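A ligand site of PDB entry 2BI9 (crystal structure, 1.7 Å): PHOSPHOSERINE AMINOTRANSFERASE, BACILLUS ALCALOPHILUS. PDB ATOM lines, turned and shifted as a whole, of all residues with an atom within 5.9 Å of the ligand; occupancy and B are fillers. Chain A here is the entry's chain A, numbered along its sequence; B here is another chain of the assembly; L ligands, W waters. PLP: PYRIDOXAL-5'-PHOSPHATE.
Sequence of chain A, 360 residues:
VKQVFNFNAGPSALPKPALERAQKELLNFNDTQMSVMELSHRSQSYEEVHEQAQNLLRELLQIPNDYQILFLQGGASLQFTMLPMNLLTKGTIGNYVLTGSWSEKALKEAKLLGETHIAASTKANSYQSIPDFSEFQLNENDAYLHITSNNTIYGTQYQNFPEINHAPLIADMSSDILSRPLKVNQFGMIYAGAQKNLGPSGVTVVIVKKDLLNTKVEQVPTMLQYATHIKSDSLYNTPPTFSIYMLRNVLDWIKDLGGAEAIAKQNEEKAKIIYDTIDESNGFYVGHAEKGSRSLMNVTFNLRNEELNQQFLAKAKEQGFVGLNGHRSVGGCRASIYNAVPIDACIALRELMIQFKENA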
ATOM      1  N   ALA A   9      14.933  18.553 -16.817  1.00  0.00           N
ATOM      2  CA  ALA A   9      15.504  17.250 -17.118  1.00  0.00           C
ATOM      3  C   ALA A   9      14.884  16.102 -16.349  1.00  0.00           C
ATOM      4  O   ALA A   9      15.208  14.923 -16.603  1.00  0.00           O
ATOM      5  CB  ALA A   9      17.022  17.287 -16.873  1.00  0.00           C
ATOM      6  N   GLY A  74      10.274   3.717  -5.934  1.00  0.00           N
ATOM      7  CA  GLY A  74      11.674   3.665  -5.546  1.00  0.00           C
ATOM      8  C   GLY A  74      12.589   4.276  -6.591  1.00  0.00           C
ATOM      9  O   GLY A  74      13.784   4.487  -6.335  1.00  0.00           O
ATOM     10  N   GLY A  75      12.000   4.537  -7.753  1.00  0.00           N
ATOM     11  CA  GLY A  75      12.808   5.174  -8.795  1.00  0.00           C
ATOM     12  C   GLY A  75      13.750   4.191  -9.475  1.00  0.00           C
ATOM     13  O   GLY A  75      13.884   3.012  -9.123  1.00  0.00           O
ATOM     14  N   ALA A  76      14.423   4.725 -10.510  1.00  0.00           N
ATOM     15  CA  ALA A  76      15.398   3.873 -11.188  1.00  0.00           C
ATOM     16  C   ALA A  76      16.503   3.506 -10.225  1.00  0.00           C
ATOM     17  O   ALA A  76      17.098   2.429 -10.273  1.00  0.00           O
ATOM     18  CB  ALA A  76      15.937   4.599 -12.418  1.00  0.00           C
ATOM     19  N   SER A  77      16.785   4.436  -9.321  1.00  0.00           N
ATOM     20  CA  SER A  77      17.844   4.215  -8.346  1.00  0.00           C
ATOM     21  C   SER A  77      17.629   2.947  -7.557  1.00  0.00           C
ATOM     22  O   SER A  77      18.590   2.218  -7.302  1.00  0.00           O
ATOM     23  CB  SER A  77      18.011   5.401  -7.385  1.00  0.00           C
ATOM     24  OG  SER A  77      18.481   6.503  -8.141  1.00  0.00           O
ATOM     25  N   LEU A  78      16.379   2.647  -7.179  1.00  0.00           N
ATOM     26  CA  LEU A  78      16.148   1.405  -6.456  1.00  0.00           C
ATOM     27  C   LEU A  78      16.403   0.208  -7.373  1.00  0.00           C
ATOM     28  O   LEU A  78      16.840  -0.849  -6.920  1.00  0.00           O
ATOM     29  CB  LEU A  78      14.734   1.324  -5.878  1.00  0.00           C
ATOM     30  CG  LEU A  78      14.479   0.066  -5.043  1.00  0.00           C
ATOM     31  CD1 LEU A  78      15.542  -0.044  -3.961  1.00  0.00           C
ATOM     32  CD2 LEU A  78      13.078   0.033  -4.453  1.00  0.00           C
ATOM     33  N   PHE A  80      18.713  -0.031  -9.504  1.00  0.00           N
ATOM     34  CA  PHE A  80      20.151  -0.292  -9.502  1.00  0.00           C
ATOM     35  C   PHE A  80      20.525  -1.386  -8.500  1.00  0.00           C
ATOM     36  O   PHE A  80      21.451  -2.166  -8.727  1.00  0.00           O
ATOM     37  CB  PHE A  80      20.956   0.963  -9.188  1.00  0.00           C
ATOM     38  CG  PHE A  80      20.881   2.102 -10.197  1.00  0.00           C
ATOM     39  CD1 PHE A  80      21.246   3.388  -9.807  1.00  0.00           C
ATOM     40  CD2 PHE A  80      20.439   1.887 -11.497  1.00  0.00           C
ATOM     41  CE1 PHE A  80      21.182   4.466 -10.703  1.00  0.00           C
ATOM     42  CE2 PHE A  80      20.418   2.932 -12.391  1.00  0.00           C
ATOM     43  CZ  PHE A  80      20.784   4.204 -12.011  1.00  0.00           C
ATOM     44  N   TRP A 102      25.024   7.817 -14.918  1.00  0.00           N
ATOM     45  CA  TRP A 102      24.004   6.858 -14.468  1.00  0.00           C
ATOM     46  C   TRP A 102      24.501   5.428 -14.637  1.00  0.00           C
ATOM     47  O   TRP A 102      24.220   4.558 -13.808  1.00  0.00           O
ATOM     48  CB  TRP A 102      22.650   7.050 -15.165  1.00  0.00           C
ATOM     49  CG  TRP A 102      22.046   8.363 -14.740  1.00  0.00           C
ATOM     50  CD1 TRP A 102      21.821   9.468 -15.502  1.00  0.00           C
ATOM     51  CD2 TRP A 102      21.604   8.684 -13.415  1.00  0.00           C
ATOM     52  NE1 TRP A 102      21.256  10.464 -14.745  1.00  0.00           N
ATOM     53  CE2 TRP A 102      21.113  10.002 -13.459  1.00  0.00           C
ATOM     54  CE3 TRP A 102      21.563   7.970 -12.205  1.00  0.00           C
ATOM     55  CZ2 TRP A 102      20.591  10.643 -12.332  1.00  0.00           C
ATOM     56  CZ3 TRP A 102      21.043   8.625 -11.098  1.00  0.00           C
ATOM     57  CH2 TRP A 102      20.567   9.937 -11.154  1.00  0.00           C
ATOM     58  N   THR A 148      22.945   1.626 -20.366  1.00  0.00           N
ATOM     59  CA  THR A 148      22.124   2.836 -20.195  1.00  0.00           C
ATOM     60  C   THR A 148      21.792   3.378 -21.576  1.00  0.00           C
ATOM     61  O   THR A 148      22.662   3.927 -22.259  1.00  0.00           O
ATOM     62  CB  THR A 148      22.877   3.840 -19.324  1.00  0.00           C
ATOM     63  OG1 THR A 148      23.383   3.111 -18.194  1.00  0.00           O
ATOM     64  CG2 THR A 148      21.957   4.951 -18.828  1.00  0.00           C
ATOM     65  N   ASN A 150      20.051   5.873 -22.835  1.00  0.00           N
ATOM     66  CA  ASN A 150      20.227   7.315 -22.984  1.00  0.00           C
ATOM     67  C   ASN A 150      20.947   7.894 -21.758  1.00  0.00           C
ATOM     68  O   ASN A 150      20.478   7.748 -20.614  1.00  0.00           O
ATOM     69  CB  ASN A 150      18.874   8.021 -23.213  1.00  0.00           C
ATOM     70  CG  ASN A 150      19.053   9.485 -23.542  1.00  0.00           C
ATOM     71  OD1 ASN A 150      18.928  10.370 -22.689  1.00  0.00           O
ATOM     72  ND2 ASN A 150      19.364   9.825 -24.775  1.00  0.00           N
ATOM     73  N   ASN A 151      22.103   8.515 -21.997  1.00  0.00           N
ATOM     74  CA  ASN A 151      22.964   8.987 -20.912  1.00  0.00           C
ATOM     75  C   ASN A 151      22.633  10.433 -20.618  1.00  0.00           C
ATOM     76  O   ASN A 151      23.170  11.350 -21.219  1.00  0.00           O
ATOM     77  CB  ASN A 151      24.432   8.746 -21.325  1.00  0.00           C
ATOM     78  CG  ASN A 151      24.621   7.291 -21.698  1.00  0.00           C
ATOM     79  OD1 ASN A 151      24.776   6.418 -20.826  1.00  0.00           O
ATOM     80  ND2 ASN A 151      24.633   6.978 -22.976  1.00  0.00           N
ATOM     81  N   THR A 152      21.682  10.568 -19.686  1.00  0.00           N
ATOM     82  CA  THR A 152      20.940  11.801 -19.456  1.00  0.00           C
ATOM     83  C   THR A 152      21.838  12.991 -19.213  1.00  0.00           C
ATOM     84  O   THR A 152      21.527  14.137 -19.577  1.00  0.00           O
ATOM     85  CB  THR A 152      20.010  11.613 -18.231  1.00  0.00           C
ATOM     86  OG1 THR A 152      19.550  10.261 -18.270  1.00  0.00           O
ATOM     87  CG2 THR A 152      18.805  12.525 -18.325  1.00  0.00           C
ATOM     88  N   ASP A 172      18.739   0.431 -18.546  1.00  0.00           N
ATOM     89  CA  ASP A 172      18.167   1.618 -17.902  1.00  0.00           C
ATOM     90  C   ASP A 172      17.727   2.570 -19.013  1.00  0.00           C
ATOM     91  O   ASP A 172      18.573   3.251 -19.615  1.00  0.00           O
ATOM     92  CB  ASP A 172      19.182   2.270 -16.972  1.00  0.00           C
ATOM     93  CG  ASP A 172      18.724   3.566 -16.349  1.00  0.00           C
ATOM     94  OD1 ASP A 172      17.571   3.990 -16.616  1.00  0.00           O
ATOM     95  OD2 ASP A 172      19.535   4.152 -15.587  1.00  0.00           O
ATOM     96  N   MET A 173      16.414   2.604 -19.261  1.00  0.00           N
ATOM     97  CA  MET A 173      15.898   3.498 -20.308  1.00  0.00           C
ATOM     98  C   MET A 173      15.149   4.706 -19.752  1.00  0.00           C
ATOM     99  O   MET A 173      14.288   5.224 -20.448  1.00  0.00           O
ATOM    100  CB  MET A 173      14.978   2.720 -21.245  1.00  0.00           C
ATOM    101  CG  MET A 173      15.737   1.629 -22.012  1.00  0.00           C
ATOM    102  SD  MET A 173      14.709   0.986 -23.356  1.00  0.00           S
ATOM    103  CE  MET A 173      15.835  -0.218 -24.086  1.00  0.00           C
ATOM    104  N   SER A 174      15.475   5.115 -18.537  1.00  0.00           N
ATOM    105  CA  SER A 174      14.774   6.218 -17.870  1.00  0.00           C
ATOM    106  C   SER A 174      14.560   7.419 -18.764  1.00  0.00           C
ATOM    107  O   SER A 174      13.453   7.958 -18.783  1.00  0.00           O
ATOM    108  CB  SER A 174      15.551   6.652 -16.622  1.00  0.00           C
ATOM    109  OG  SER A 174      15.587   5.604 -15.656  1.00  0.00           O
ATOM    110  N   SER A 175      15.608   7.847 -19.517  1.00  0.00           N
ATOM    111  CA  SER A 175      15.383   9.114 -20.232  1.00  0.00           C
ATOM    112  C   SER A 175      15.092   8.939 -21.713  1.00  0.00           C
ATOM    113  O   SER A 175      15.067   9.973 -22.402  1.00  0.00           O
ATOM    114  CB  SER A 175      16.577  10.071 -20.009  1.00  0.00           C
ATOM    115  OG  SER A 175      17.805   9.392 -20.212  1.00  0.00           O
ATOM    116  N   TYR A 191      14.071  -0.916 -17.570  1.00  0.00           N
ATOM    117  CA  TYR A 191      13.417  -0.140 -16.489  1.00  0.00           C
ATOM    118  C   TYR A 191      13.595   1.346 -16.742  1.00  0.00           C
ATOM    119  O   TYR A 191      14.523   1.763 -17.425  1.00  0.00           O
ATOM    120  CB  TYR A 191      13.934  -0.587 -15.131  1.00  0.00           C
ATOM    121  CG  TYR A 191      15.399  -0.341 -14.880  1.00  0.00           C
ATOM    122  CD1 TYR A 191      15.849   0.835 -14.311  1.00  0.00           C
ATOM    123  CD2 TYR A 191      16.350  -1.310 -15.194  1.00  0.00           C
ATOM    124  CE1 TYR A 191      17.187   1.061 -14.064  1.00  0.00           C
ATOM    125  CE2 TYR A 191      17.703  -1.090 -14.958  1.00  0.00           C
ATOM    126  CZ  TYR A 191      18.117   0.088 -14.386  1.00  0.00           C
ATOM    127  OH  TYR A 191      19.440   0.371 -14.133  1.00  0.00           O
ATOM    128  N   GLY A 193      12.484   5.186 -14.556  1.00  0.00           N
ATOM    129  CA  GLY A 193      11.658   6.053 -13.708  1.00  0.00           C
ATOM    130  C   GLY A 193      10.710   6.770 -14.659  1.00  0.00           C
ATOM    131  O   GLY A 193      11.051   7.193 -15.770  1.00  0.00           O
ATOM    132  N   GLN A 195       9.409   9.767 -14.577  1.00  0.00           N
ATOM    133  CA  GLN A 195       9.402  11.221 -14.580  1.00  0.00           C
ATOM    134  C   GLN A 195      10.189  11.834 -15.706  1.00  0.00           C
ATOM    135  O   GLN A 195      10.281  13.065 -15.820  1.00  0.00           O
ATOM    136  CB  GLN A 195       9.956  11.763 -13.245  1.00  0.00           C
ATOM    137  CG  GLN A 195      11.433  11.459 -13.036  1.00  0.00           C
ATOM    138  CD  GLN A 195      11.685  10.116 -12.371  1.00  0.00           C
ATOM    139  OE1 GLN A 195      10.856   9.209 -12.327  1.00  0.00           O
ATOM    140  NE2 GLN A 195      12.896   9.978 -11.835  1.00  0.00           N
ATOM    141  N   LYS A 196      10.793  11.056 -16.614  1.00  0.00           N
ATOM    142  CA  LYS A 196      11.464  11.869 -17.659  1.00  0.00           C
ATOM    143  C   LYS A 196      10.631  11.890 -18.912  1.00  0.00           C
ATOM    144  O   LYS A 196      10.370  12.888 -19.570  1.00  0.00           O
ATOM    145  CB  LYS A 196      12.884  11.333 -17.897  1.00  0.00           C
ATOM    146  CG  LYS A 196      13.596  11.009 -16.596  1.00  0.00           C
ATOM    147  CD  LYS A 196      15.085  11.303 -16.694  1.00  0.00           C
ATOM    148  CE  LYS A 196      15.620  11.845 -15.385  1.00  0.00           C
ATOM    149  NZ  LYS A 196      16.637  10.949 -14.776  1.00  0.00           N
ATOM    150  N   THR A 204       8.004   3.710 -11.208  1.00  0.00           N
ATOM    151  CA  THR A 204       9.080   3.209 -12.049  1.00  0.00           C
ATOM    152  C   THR A 204       8.520   2.070 -12.898  1.00  0.00           C
ATOM    153  O   THR A 204       7.942   1.156 -12.318  1.00  0.00           O
ATOM    154  CB  THR A 204      10.269   2.703 -11.203  1.00  0.00           C
ATOM    155  OG1 THR A 204      10.846   3.832 -10.533  1.00  0.00           O
ATOM    156  CG2 THR A 204      11.344   2.117 -12.093  1.00  0.00           C
ATOM    157  N   TYR A 338      12.409  15.821 -24.126  1.00  0.00           N
ATOM    158  CA  TYR A 338      11.596  14.614 -24.045  1.00  0.00           C
ATOM    159  C   TYR A 338      10.329  14.727 -24.901  1.00  0.00           C
ATOM    160  O   TYR A 338      10.045  15.812 -25.405  1.00  0.00           O
ATOM    161  CB  TYR A 338      11.214  14.361 -22.586  1.00  0.00           C
ATOM    162  CG  TYR A 338      12.405  14.233 -21.669  1.00  0.00           C
ATOM    163  CD1 TYR A 338      12.589  15.110 -20.613  1.00  0.00           C
ATOM    164  CD2 TYR A 338      13.337  13.222 -21.852  1.00  0.00           C
ATOM    165  CE1 TYR A 338      13.671  15.001 -19.761  1.00  0.00           C
ATOM    166  CE2 TYR A 338      14.426  13.106 -20.989  1.00  0.00           C
ATOM    167  CZ  TYR A 338      14.598  13.996 -19.955  1.00  0.00           C
ATOM    168  OH  TYR A 338      15.672  13.904 -19.088  1.00  0.00           O
ATOM    169  N   HIS B  41      13.055  18.339  -9.268  1.00  0.00           N
ATOM    170  CA  HIS B  41      13.126  18.245  -7.817  1.00  0.00           C
ATOM    171  C   HIS B  41      14.293  19.048  -7.268  1.00  0.00           C
ATOM    172  O   HIS B  41      14.439  19.210  -6.058  1.00  0.00           O
ATOM    173  CB  HIS B  41      13.215  16.788  -7.381  1.00  0.00           C
ATOM    174  CG  HIS B  41      14.403  16.073  -7.928  1.00  0.00           C
ATOM    175  ND1 HIS B  41      14.660  15.923  -9.267  1.00  0.00           N
ATOM    176  CD2 HIS B  41      15.433  15.457  -7.274  1.00  0.00           C
ATOM    177  CE1 HIS B  41      15.785  15.250  -9.436  1.00  0.00           C
ATOM    178  NE2 HIS B  41      16.272  14.953  -8.237  1.00  0.00           N
ATOM    179  N   GLN B  73       9.972   6.390  -0.689  1.00  0.00           N
ATOM    180  CA  GLN B  73       9.062   5.614  -1.495  1.00  0.00           C
ATOM    181  C   GLN B  73       9.024   4.176  -0.995  1.00  0.00           C
ATOM    182  O   GLN B  73       9.878   3.824  -0.162  1.00  0.00           O
ATOM    183  CB  GLN B  73       9.526   5.633  -2.963  1.00  0.00           C
ATOM    184  CG  GLN B  73       9.472   7.021  -3.613  1.00  0.00           C
ATOM    185  CD  GLN B  73       9.868   6.898  -5.089  1.00  0.00           C
ATOM    186  OE1 GLN B  73       9.123   6.280  -5.869  1.00  0.00           O
ATOM    187  NE2 GLN B  73      11.026   7.454  -5.431  1.00  0.00           N
ATOM    188  N   ASN B 237      17.605  10.773  -4.595  1.00  0.00           N
ATOM    189  CA  ASN B 237      17.091  10.547  -5.952  1.00  0.00           C
ATOM    190  C   ASN B 237      15.783  11.331  -6.071  1.00  0.00           C
ATOM    191  O   ASN B 237      15.460  12.140  -5.204  1.00  0.00           O
ATOM    192  CB  ASN B 237      16.896   9.085  -6.313  1.00  0.00           C
ATOM    193  CG  ASN B 237      15.765   8.395  -5.618  1.00  0.00           C
ATOM    194  OD1 ASN B 237      15.451   8.698  -4.458  1.00  0.00           O
ATOM    195  ND2 ASN B 237      15.169   7.468  -6.352  1.00  0.00           N
ATOM    196  N   THR B 238      15.059  11.120  -7.146  1.00  0.00           N
ATOM    197  CA  THR B 238      13.864  11.915  -7.413  1.00  0.00           C
ATOM    198  C   THR B 238      12.774  11.489  -6.426  1.00  0.00           C
ATOM    199  O   THR B 238      12.406  10.311  -6.407  1.00  0.00           O
ATOM    200  CB  THR B 238      13.378  11.720  -8.850  1.00  0.00           C
ATOM    201  OG1 THR B 238      14.460  11.896  -9.786  1.00  0.00           O
ATOM    202  CG2 THR B 238      12.315  12.774  -9.215  1.00  0.00           C
HETATM  203  N1  PLP L   1      18.854   6.578 -14.640  1.00  0.00           N
HETATM  204  C2  PLP L   1      18.771   7.547 -15.616  1.00  0.00           C
HETATM  205  C2A PLP L   1      19.250   7.290 -17.042  1.00  0.00           C
HETATM  206  C3  PLP L   1      18.268   8.777 -15.277  1.00  0.00           C
HETATM  207  O3  PLP L   1      18.216   9.725 -16.272  1.00  0.00           O
HETATM  208  C4  PLP L   1      17.900   9.022 -13.974  1.00  0.00           C
HETATM  209  C4A PLP L   1      17.235  10.362 -13.589  1.00  0.00           C
HETATM  210  C5  PLP L   1      17.964   8.036 -13.016  1.00  0.00           C
HETATM  211  C6  PLP L   1      18.501   6.818 -13.349  1.00  0.00           C
HETATM  212  C5A PLP L   1      17.504   8.301 -11.568  1.00  0.00           C
HETATM  213  O4P PLP L   1      16.123   8.004 -11.396  1.00  0.00           O
HETATM  214  P   PLP L   1      15.410   8.171  -9.962  1.00  0.00           P
HETATM  215  O1P PLP L   1      15.741   9.558  -9.594  1.00  0.00           O
HETATM  216  O2P PLP L   1      16.077   7.132  -9.147  1.00  0.00           O
HETATM  217  O3P PLP L   1      13.991   7.909 -10.248  1.00  0.00           O
HETATM  218  O   HOH W   1      12.230   8.290  -8.163  1.00  0.00           O
HETATM  219  O   HOH W   2      14.457   7.401 -13.629  1.00  0.00           O
HETATM  220  O   HOH W   3      18.018  10.855  -8.996  1.00  0.00           O
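Merely in contact with the ligand: Gly 75 (3.3 Å), Ser 174 (3.5 Å), Phe 80 (3.7 Å), Asn 150 (3.8 Å), Ser 175 (3.98 Å) and Thr 148 (3.999 Å). Hydrophobic or aromatic side chains that line the ligand: Ala 76, Phe 80 and Trp 102. Of the 26 residues printed, 15 come within 4 Å of the ligand. Along chain A the residues within 4 Å of the ligand span positions 75 to 196. The nearest printed residue that does not touch the ligand is Gly 74 (4.5 Å).
Water W3 lies within hydrogen-bond range of O1P of the ligand and N of Thr 238 of chain B. Water W1 lies within hydrogen-bond range of the backbone carbonyl oxygen (O) of Thr 238 of chain B (2.7 Å), an oxygen (O3P) of the ligand (2.8 Å) and the side-chain amide nitrogen (NE2) of Gln 73 of chain B (3.1 Å). Water W2 lies within hydrogen-bond range of an oxygen (O4P) of the ligand (2.9 Å), the side-chain hydroxyl of Ser 174 (2.9 Å) and the backbone NH of Gly 193 (3.1 Å).
C4A of the ligand is bonded to NZ of Lys 196 (1.5 Å). The side-chain hydroxyl (OG1) of Thr 152 sits at hydrogen-bond distance from an oxygen (O3) of the ligand (2.5 Å). N of Thr 238 of chain B sits at hydrogen-bond distance from O1P of the ligand (3.0 Å). An oxygen (O1P) of the ligand is in hydrogen-bond range of the side-chain hydroxyl (OG1) of Thr 238 of chain B (2.7 Å). N of Ser 77 lies within hydrogen-bond range of O2P of the ligand (2.8 Å). An oxygen (O2P) of the ligand sits at hydrogen-bond distance from the side-chain hydroxyl (OG) of Ser 77, at 2.7 Å. A nitrogen (N1) of the ligand is in hydrogen-bond range of the side-chain carboxylate (OD2) of Asp 172, at 2.7 Å. The side-chain amide nitrogen (NE2) of Gln 195 sits at hydrogen-bond distance from an oxygen (O3P) of the ligand, 2.8 Å away. O2P of the ligand is in hydrogen-bond range of ND2 of Asn 237 of chain B (3.0 Å). The backbone NH of Ala 76 lies within hydrogen-bond range of an oxygen (O2P) of the ligand (3.2 Å). O3 of the ligand sits close to NE1 of Trp 102, at 3.5 Å.
OG1 of Thr 152 sits at hydrogen-bond distance from OG of Ser 175, at 2.8 Å. The side-chain amide nitrogen of Gln 195 sits at hydrogen-bond distance from the side-chain hydroxyl of Thr 238 of chain B, at 3.2 Å. The side-chain amide nitrogen (NE2) of Gln 73 of chain B lies within hydrogen-bond range of the backbone carbonyl oxygen (O) of Thr 238 of chain B, 3.3 Å away. The side-chain hydroxyl (OG) of Ser 174 sits at hydrogen-bond distance from the side-chain carboxylate (OD1) of Asp 172, 2.7 Å away. The backbone carbonyl oxygen (O) of Gly 74 sits at hydrogen-bond distance from the side-chain amide nitrogen (ND2) of Asn 237 of chain B, at 3.3 Å. N of Gly 75 lies close to OG1 of Thr 204 (3.1 Å). OG of Ser 174 is in hydrogen-bond range of N of Gly 193 (3.3 Å). OD1 of Asn 150 lies within hydrogen-bond range of OG of Ser 175 (2.9 Å).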
